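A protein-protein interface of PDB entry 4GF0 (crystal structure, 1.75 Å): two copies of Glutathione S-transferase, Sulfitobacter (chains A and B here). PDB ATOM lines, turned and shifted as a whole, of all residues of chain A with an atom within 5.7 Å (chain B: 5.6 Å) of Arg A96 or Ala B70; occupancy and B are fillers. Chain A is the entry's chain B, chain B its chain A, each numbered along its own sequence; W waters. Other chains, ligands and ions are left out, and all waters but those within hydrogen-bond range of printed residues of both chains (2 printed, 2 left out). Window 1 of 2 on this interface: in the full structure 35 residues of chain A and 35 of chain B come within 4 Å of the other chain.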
ATOM      1  N   ASP A  73      14.713   1.464   4.271  1.00  0.00           N
ATOM      2  CA  ASP A  73      14.568   0.775   5.557  1.00  0.00           C
ATOM      3  C   ASP A  73      13.134   0.912   6.081  1.00  0.00           C
ATOM      4  O   ASP A  73      12.603  -0.021   6.682  1.00  0.00           O
ATOM      5  CB  ASP A  73      15.588   1.287   6.598  1.00  0.00           C
ATOM      6  CG  ASP A  73      16.697   0.266   6.909  1.00  0.00           C
ATOM      7  OD1 ASP A  73      16.410  -0.934   7.169  1.00  0.00           O
ATOM      8  OD2 ASP A  73      17.874   0.673   6.917  1.00  0.00           O
ATOM      9  N   VAL A  85      15.393  -7.189   4.565  1.00  0.00           N
ATOM     10  CA  VAL A  85      16.606  -6.983   5.353  1.00  0.00           C
ATOM     11  C   VAL A  85      16.905  -8.285   6.075  1.00  0.00           C
ATOM     12  O   VAL A  85      15.996  -8.886   6.653  1.00  0.00           O
ATOM     13  CB  VAL A  85      16.418  -5.867   6.403  1.00  0.00           C
ATOM     14  CG1 VAL A  85      17.678  -5.697   7.248  1.00  0.00           C
ATOM     15  CG2 VAL A  85      16.062  -4.543   5.717  1.00  0.00           C
ATOM     16  N   ALA A  91      24.936  -9.446   8.438  1.00  0.00           N
ATOM     17  CA  ALA A  91      24.538  -9.347   7.038  1.00  0.00           C
ATOM     18  C   ALA A  91      23.746  -8.060   6.815  1.00  0.00           C
ATOM     19  O   ALA A  91      23.883  -7.400   5.777  1.00  0.00           O
ATOM     20  CB  ALA A  91      23.709 -10.569   6.639  1.00  0.00           C
ATOM     21  N   ALA A  92      22.907  -7.693   7.779  1.00  0.00           N
ATOM     22  CA  ALA A  92      22.157  -6.441   7.646  1.00  0.00           C
ATOM     23  C   ALA A  92      23.090  -5.221   7.578  1.00  0.00           C
ATOM     24  O   ALA A  92      22.838  -4.267   6.822  1.00  0.00           O
ATOM     25  CB  ALA A  92      21.156  -6.302   8.787  1.00  0.00           C
ATOM     26  N   ALA A  93      24.161  -5.249   8.368  1.00  0.00           N
ATOM     27  CA  ALA A  93      25.163  -4.183   8.376  1.00  0.00           C
ATOM     28  C   ALA A  93      25.934  -4.153   7.053  1.00  0.00           C
ATOM     29  O   ALA A  93      26.277  -3.079   6.551  1.00  0.00           O
ATOM     30  CB  ALA A  93      26.126  -4.367   9.544  1.00  0.00           C
ATOM     31  N   GLN A  94      26.197  -5.324   6.482  1.00  0.00           N
ATOM     32  CA  GLN A  94      26.855  -5.384   5.172  1.00  0.00           C
ATOM     33  C   GLN A  94      25.956  -4.781   4.095  1.00  0.00           C
ATOM     34  O   GLN A  94      26.423  -4.083   3.189  1.00  0.00           O
ATOM     35  CB  GLN A  94      27.276  -6.825   4.848  1.00  0.00           C
ATOM     36  CG  GLN A  94      28.349  -7.316   5.807  1.00  0.00           C
ATOM     37  CD  GLN A  94      28.603  -8.804   5.729  1.00  0.00           C
ATOM     38  OE1 GLN A  94      27.672  -9.604   5.581  1.00  0.00           O
ATOM     39  NE2 GLN A  94      29.880  -9.191   5.854  1.00  0.00           N
ATOM     40  N   MET A  95      24.661  -5.056   4.202  1.00  0.00           N
ATOM     41  CA  MET A  95      23.668  -4.461   3.307  1.00  0.00           C
ATOM     42  C   MET A  95      23.663  -2.944   3.449  1.00  0.00           C
ATOM     43  O   MET A  95      23.705  -2.204   2.457  1.00  0.00           O
ATOM     44  CB  MET A  95      22.275  -5.020   3.637  1.00  0.00           C
ATOM     45  CG  MET A  95      21.124  -4.432   2.812  1.00  0.00           C
ATOM     46  SD  MET A  95      19.534  -4.656   3.656  1.00  0.00           S
ATOM     47  CE  MET A  95      19.677  -3.426   4.965  1.00  0.00           C
ATOM     48  N   ARG A  96      23.607  -2.458   4.685  1.00  0.00           N
ATOM     49  CA  ARG A  96      23.597  -1.012   4.905  1.00  0.00           C
ATOM     50  C   ARG A  96      24.912  -0.349   4.543  1.00  0.00           C
ATOM     51  O   ARG A  96      24.928   0.809   4.116  1.00  0.00           O
ATOM     52  CB  ARG A  96      23.219  -0.671   6.351  1.00  0.00           C
ATOM     53  CG  ARG A  96      21.775  -1.024   6.667  1.00  0.00           C
ATOM     54  CD  ARG A  96      21.269  -0.325   7.919  1.00  0.00           C
ATOM     55  NE  ARG A  96      19.903  -0.774   8.203  1.00  0.00           N
ATOM     56  CZ  ARG A  96      19.591  -1.808   8.977  1.00  0.00           C
ATOM     57  NH1 ARG A  96      20.540  -2.505   9.601  1.00  0.00           N
ATOM     58  NH2 ARG A  96      18.316  -2.136   9.141  1.00  0.00           N
ATOM     59  N   SER A  97      26.010  -1.081   4.687  1.00  0.00           N
ATOM     60  CA  SER A  97      27.311  -0.527   4.312  1.00  0.00           C
ATOM     61  C   SER A  97      27.294  -0.190   2.830  1.00  0.00           C
ATOM     62  O   SER A  97      27.777   0.872   2.401  1.00  0.00           O
ATOM     63  CB  SER A  97      28.428  -1.538   4.591  1.00  0.00           C
ATOM     64  OG  SER A  97      29.690  -0.974   4.252  1.00  0.00           O
ATOM     65  N   ALA A  98      26.720  -1.090   2.043  1.00  0.00           N
ATOM     66  CA  ALA A  98      26.602  -0.859   0.609  1.00  0.00           C
ATOM     67  C   ALA A  98      25.732   0.362   0.337  1.00  0.00           C
ATOM     68  O   ALA A  98      26.044   1.194  -0.515  1.00  0.00           O
ATOM     69  CB  ALA A  98      26.032  -2.099  -0.092  1.00  0.00           C
ATOM     70  N   MET A  99      24.633   0.478   1.074  1.00  0.00           N
ATOM     71  CA  MET A  99      23.724   1.606   0.898  1.00  0.00           C
ATOM     72  C   MET A  99      24.366   2.949   1.261  1.00  0.00           C
ATOM     73  O   MET A  99      24.240   3.930   0.518  1.00  0.00           O
ATOM     74  CB  MET A  99      22.436   1.366   1.704  1.00  0.00           C
ATOM     75  CG  MET A  99      21.607   0.188   1.174  1.00  0.00           C
ATOM     76  SD  MET A  99      20.482  -0.469   2.444  1.00  0.00           S
ATOM     77  CE  MET A  99      19.276   0.861   2.466  1.00  0.00           C
ATOM     78  N   TYR A 100      25.068   3.004   2.385  1.00  0.00           N
ATOM     79  CA  TYR A 100      25.756   4.247   2.749  1.00  0.00           C
ATOM     80  C   TYR A 100      26.920   4.554   1.819  1.00  0.00           C
ATOM     81  O   TYR A 100      27.243   5.721   1.582  1.00  0.00           O
ATOM     82  CB  TYR A 100      26.238   4.220   4.203  1.00  0.00           C
ATOM     83  CG  TYR A 100      25.152   4.569   5.201  1.00  0.00           C
ATOM     84  CD1 TYR A 100      24.869   5.894   5.508  1.00  0.00           C
ATOM     85  CD2 TYR A 100      24.401   3.577   5.821  1.00  0.00           C
ATOM     86  CE1 TYR A 100      23.871   6.229   6.420  1.00  0.00           C
ATOM     87  CE2 TYR A 100      23.400   3.905   6.744  1.00  0.00           C
ATOM     88  CZ  TYR A 100      23.149   5.228   7.038  1.00  0.00           C
ATOM     89  OH  TYR A 100      22.169   5.549   7.957  1.00  0.00           O
ATOM     90  N   TYR A 101      27.563   3.520   1.291  1.00  0.00           N
ATOM     91  CA  TYR A 101      28.624   3.769   0.313  1.00  0.00           C
ATOM     92  C   TYR A 101      28.042   4.442  -0.919  1.00  0.00           C
ATOM     93  O   TYR A 101      28.620   5.390  -1.470  1.00  0.00           O
ATOM     94  CB  TYR A 101      29.332   2.473  -0.084  1.00  0.00           C
ATOM     95  CG  TYR A 101      30.354   2.672  -1.182  1.00  0.00           C
ATOM     96  CD1 TYR A 101      31.651   3.071  -0.889  1.00  0.00           C
ATOM     97  CD2 TYR A 101      30.015   2.457  -2.513  1.00  0.00           C
ATOM     98  CE1 TYR A 101      32.597   3.247  -1.905  1.00  0.00           C
ATOM     99  CE2 TYR A 101      30.944   2.644  -3.532  1.00  0.00           C
ATOM    100  CZ  TYR A 101      32.233   3.029  -3.218  1.00  0.00           C
ATOM    101  OH  TYR A 101      33.158   3.204  -4.232  1.00  0.00           O
ATOM    102  N   ALA A 162      19.738  -3.339  -0.457  1.00  0.00           N
ATOM    103  CA  ALA A 162      20.903  -2.766  -1.142  1.00  0.00           C
ATOM    104  C   ALA A 162      20.762  -2.854  -2.654  1.00  0.00           C
ATOM    105  O   ALA A 162      21.359  -2.068  -3.399  1.00  0.00           O
ATOM    106  CB  ALA A 162      22.191  -3.446  -0.687  1.00  0.00           C
ATOM    107  N   THR B  66      32.233  -1.422   7.448  1.00  0.00           N
ATOM    108  CA  THR B  66      32.530  -0.012   7.197  1.00  0.00           C
ATOM    109  C   THR B  66      31.250   0.782   7.002  1.00  0.00           C
ATOM    110  O   THR B  66      30.175   0.192   6.826  1.00  0.00           O
ATOM    111  CB  THR B  66      33.384   0.192   5.936  1.00  0.00           C
ATOM    112  OG1 THR B  66      32.667  -0.291   4.790  1.00  0.00           O
ATOM    113  CG2 THR B  66      34.713  -0.555   6.059  1.00  0.00           C
ATOM    114  N   GLU B  67      31.416   2.111   6.987  1.00  0.00           N
ATOM    115  CA  GLU B  67      30.367   3.138   6.806  1.00  0.00           C
ATOM    116  C   GLU B  67      29.672   3.478   8.112  1.00  0.00           C
ATOM    117  O   GLU B  67      28.938   2.667   8.676  1.00  0.00           O
ATOM    118  CB  GLU B  67      29.339   2.796   5.719  1.00  0.00           C
ATOM    119  CG  GLU B  67      29.940   2.594   4.325  1.00  0.00           C
ATOM    120  CD  GLU B  67      30.496   3.872   3.712  1.00  0.00           C
ATOM    121  OE1 GLU B  67      30.053   4.983   4.095  1.00  0.00           O
ATOM    122  OE2 GLU B  67      31.374   3.765   2.828  1.00  0.00           O
ATOM    123  N   THR B  68      29.909   4.697   8.578  1.00  0.00           N
ATOM    124  CA  THR B  68      29.411   5.131   9.877  1.00  0.00           C
ATOM    125  C   THR B  68      27.947   4.745  10.126  1.00  0.00           C
ATOM    126  O   THR B  68      27.624   4.158  11.161  1.00  0.00           O
ATOM    127  CB  THR B  68      29.593   6.644  10.015  1.00  0.00           C
ATOM    128  OG1 THR B  68      30.991   6.949   9.908  1.00  0.00           O
ATOM    129  CG2 THR B  68      29.079   7.145  11.370  1.00  0.00           C
ATOM    130  N   GLY B  69      27.060   5.049   9.183  1.00  0.00           N
ATOM    131  CA  GLY B  69      25.644   4.805   9.413  1.00  0.00           C
ATOM    132  C   GLY B  69      25.334   3.331   9.591  1.00  0.00           C
ATOM    133  O   GLY B  69      24.460   2.954  10.381  1.00  0.00           O
ATOM    134  N   ALA B  70      26.041   2.485   8.845  1.00  0.00           N
ATOM    135  CA  ALA B  70      25.854   1.040   8.948  1.00  0.00           C
ATOM    136  C   ALA B  70      26.352   0.542  10.299  1.00  0.00           C
ATOM    137  O   ALA B  70      25.724  -0.312  10.934  1.00  0.00           O
ATOM    138  CB  ALA B  70      26.587   0.320   7.798  1.00  0.00           C
ATOM    139  N   LEU B  71      27.476   1.087  10.754  1.00  0.00           N
ATOM    140  CA  LEU B  71      28.033   0.687  12.050  1.00  0.00           C
ATOM    141  C   LEU B  71      27.131   1.115  13.193  1.00  0.00           C
ATOM    142  O   LEU B  71      27.022   0.420  14.189  1.00  0.00           O
ATOM    143  CB  LEU B  71      29.407   1.324  12.263  1.00  0.00           C
ATOM    144  CG  LEU B  71      30.491   0.951  11.251  1.00  0.00           C
ATOM    145  CD1 LEU B  71      31.871   1.383  11.733  1.00  0.00           C
ATOM    146  CD2 LEU B  71      30.456  -0.515  11.019  1.00  0.00           C
ATOM    147  N   LEU B  72      26.521   2.288  13.068  1.00  0.00           N
ATOM    148  CA  LEU B  72      25.593   2.762  14.102  1.00  0.00           C
ATOM    149  C   LEU B  72      24.379   1.833  14.205  1.00  0.00           C
ATOM    150  O   LEU B  72      23.986   1.413  15.302  1.00  0.00           O
ATOM    151  CB  LEU B  72      25.159   4.206  13.811  1.00  0.00           C
ATOM    152  CG  LEU B  72      26.218   5.294  14.024  1.00  0.00           C
ATOM    153  CD1 LEU B  72      25.728   6.653  13.462  1.00  0.00           C
ATOM    154  CD2 LEU B  72      26.536   5.416  15.501  1.00  0.00           C
ATOM    155  N   ASP B  73      23.776   1.485  13.074  1.00  0.00           N
ATOM    156  CA  ASP B  73      22.664   0.532  13.108  1.00  0.00           C
ATOM    157  C   ASP B  73      23.106  -0.833  13.639  1.00  0.00           C
ATOM    158  O   ASP B  73      22.345  -1.514  14.322  1.00  0.00           O
ATOM    159  CB  ASP B  73      21.989   0.403  11.727  1.00  0.00           C
ATOM    160  CG  ASP B  73      20.618   1.059  11.691  1.00  0.00           C
ATOM    161  OD1 ASP B  73      19.813   0.803  12.616  1.00  0.00           O
ATOM    162  OD2 ASP B  73      20.346   1.844  10.754  1.00  0.00           O
ATOM    163  N   TYR B  74      24.339  -1.234  13.342  1.00  0.00           N
ATOM    164  CA  TYR B  74      24.850  -2.497  13.875  1.00  0.00           C
ATOM    165  C   TYR B  74      24.933  -2.482  15.409  1.00  0.00           C
ATOM    166  O   TYR B  74      24.496  -3.426  16.087  1.00  0.00           O
ATOM    167  CB  TYR B  74      26.215  -2.858  13.256  1.00  0.00           C
ATOM    168  CG  TYR B  74      26.710  -4.175  13.803  1.00  0.00           C
ATOM    169  CD1 TYR B  74      26.230  -5.369  13.301  1.00  0.00           C
ATOM    170  CD2 TYR B  74      27.629  -4.219  14.841  1.00  0.00           C
ATOM    171  CE1 TYR B  74      26.656  -6.590  13.818  1.00  0.00           C
ATOM    172  CE2 TYR B  74      28.048  -5.439  15.374  1.00  0.00           C
ATOM    173  CZ  TYR B  74      27.566  -6.607  14.851  1.00  0.00           C
ATOM    174  OH  TYR B  74      27.966  -7.819  15.374  1.00  0.00           O
ATOM    175  N   VAL B  75      25.486  -1.408  15.959  1.00  0.00           N
ATOM    176  CA  VAL B  75      25.582  -1.271  17.409  1.00  0.00           C
ATOM    177  C   VAL B  75      24.210  -1.347  18.065  1.00  0.00           C
ATOM    178  O   VAL B  75      24.025  -2.025  19.074  1.00  0.00           O
ATOM    179  CB  VAL B  75      26.301   0.022  17.806  1.00  0.00           C
ATOM    180  CG1 VAL B  75      26.192   0.232  19.336  1.00  0.00           C
ATOM    181  CG2 VAL B  75      27.758  -0.084  17.386  1.00  0.00           C
ATOM    182  N   ARG B  96      16.825   7.842  10.510  1.00  0.00           N
ATOM    183  CA  ARG B  96      17.695   7.455   9.395  1.00  0.00           C
ATOM    184  C   ARG B  96      17.790   8.524   8.319  1.00  0.00           C
ATOM    185  O   ARG B  96      18.807   8.621   7.634  1.00  0.00           O
ATOM    186  CB  ARG B  96      17.296   6.095   8.800  1.00  0.00           C
ATOM    187  CG  ARG B  96      17.645   4.939   9.736  1.00  0.00           C
ATOM    188  CD  ARG B  96      17.574   3.590   9.044  1.00  0.00           C
ATOM    189  NE  ARG B  96      17.750   2.544  10.050  1.00  0.00           N
ATOM    190  CZ  ARG B  96      16.747   1.920  10.661  1.00  0.00           C
ATOM    191  NH1 ARG B  96      15.487   2.201  10.340  1.00  0.00           N
ATOM    192  NH2 ARG B  96      17.009   1.010  11.596  1.00  0.00           N
ATOM    193  N   TYR B 100      21.308   9.647   6.813  1.00  0.00           N
ATOM    194  CA  TYR B 100      21.670   9.675   5.399  1.00  0.00           C
ATOM    195  C   TYR B 100      21.948  11.085   4.912  1.00  0.00           C
ATOM    196  O   TYR B 100      22.796  11.269   4.042  1.00  0.00           O
ATOM    197  CB  TYR B 100      20.612   8.999   4.528  1.00  0.00           C
ATOM    198  CG  TYR B 100      20.776   7.494   4.469  1.00  0.00           C
ATOM    199  CD1 TYR B 100      21.602   6.905   3.524  1.00  0.00           C
ATOM    200  CD2 TYR B 100      20.103   6.667   5.357  1.00  0.00           C
ATOM    201  CE1 TYR B 100      21.759   5.528   3.459  1.00  0.00           C
ATOM    202  CE2 TYR B 100      20.257   5.285   5.309  1.00  0.00           C
ATOM    203  CZ  TYR B 100      21.080   4.728   4.352  1.00  0.00           C
ATOM    204  OH  TYR B 100      21.221   3.369   4.286  1.00  0.00           O
HETATM  205  O   HOH W   1      23.436  -2.119  10.174  1.00  0.00           O
HETATM  206  O   HOH W   2      30.872  -3.368   5.526  1.00  0.00           O
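O of Thr B66 lies within hydrogen-bond range of OG of Ser A97.
The guanidinium group (NE) of Arg A96 is in salt-bridge range of the side-chain carboxylate (OD2) of Asp B73, at 3.7 Å.
The guanidinium group (NE) of Arg B96 lies within salt-bridge range of the side-chain carboxylate (OD2) of Asp A73.
NE of Arg B96 is in salt-bridge range of OD2 of Asp B73.
The side-chain carboxylate (OD2) of Asp A73 is in salt-bridge range of the guanidinium group (NE) of Arg A96 (2.8 Å).
Among the printed residues, pairs that only touch across the chains: Ala A93 with Ala B70 (3.6 Å), Ala A93 with Tyr B74 (3.9 Å), Arg A96 with Ala B70 (3.7 Å), Ser A97 with Glu B67 (3.4 Å), Ser A97 with Ala B70 (3.5 Å), Met A99 with Tyr B100 (3.5 Å), Tyr A100 with Glu B67 (3.7 Å), Tyr A100 with Gly B69 (3.5 Å), Tyr A100 with Ala B70 (3.6 Å), Tyr A100 with Tyr B100 (3.3 Å) and Tyr A101 with Glu B67 (3.7 Å).
Arg A96 touches two residues of chain B.
Ala B70 touches just these residues of chain A: Ala A93, Arg A96, Ser A97 and Tyr A100.
Printed residues of chain A within 4 Å of Gly B69: Tyr A100 (3.5 Å).
Printed residues of chain B within 4 Å of Tyr A101: Glu B67 (3.7 Å).
Printed residues of chain A within 4 Å of Glu B67: Ser A97, Tyr A100 and Tyr A101.
Of the printed residues of chain A, Tyr B74 touches Ala A93 (3.9 Å).
Val B75 touches none of the printed residues of chain A.
The nearest residue of chain B that does not touch Arg A96 is Arg B96 (4.2 Å).
The nearest printed residue of chain A that does not touch Gly B69 is Arg A96 (5.2 Å).
Hydrophobic or aromatic side chains of chain A that line the printed part of chain B: Ala A93, Met A99, Tyr A100 and Tyr A101.
Among the printed residues, 14 pairs touch across the chains.
Among the printed residues, Asp or Glu carboxylates within 4 Å of a Lys or Arg side-chain nitrogen of the other chain: Asp A73 with Arg B96 (3.7 Å) and Arg A96 with Asp B73 (3.7 Å).
Asp A73 touches Arg B96, and with the chains exchanged Arg A96 touches Asp B73.
Tyr B100 touches its own counterpart, Tyr A100.
Water W2 bridges OG of Ser A97 and N of Thr B66.
Water W1 lies within hydrogen-bond range of NH1 of Arg A96 (3.0 Å), O of Ala B70 (3.0 Å) and N of Tyr B74 (3.4 Å).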
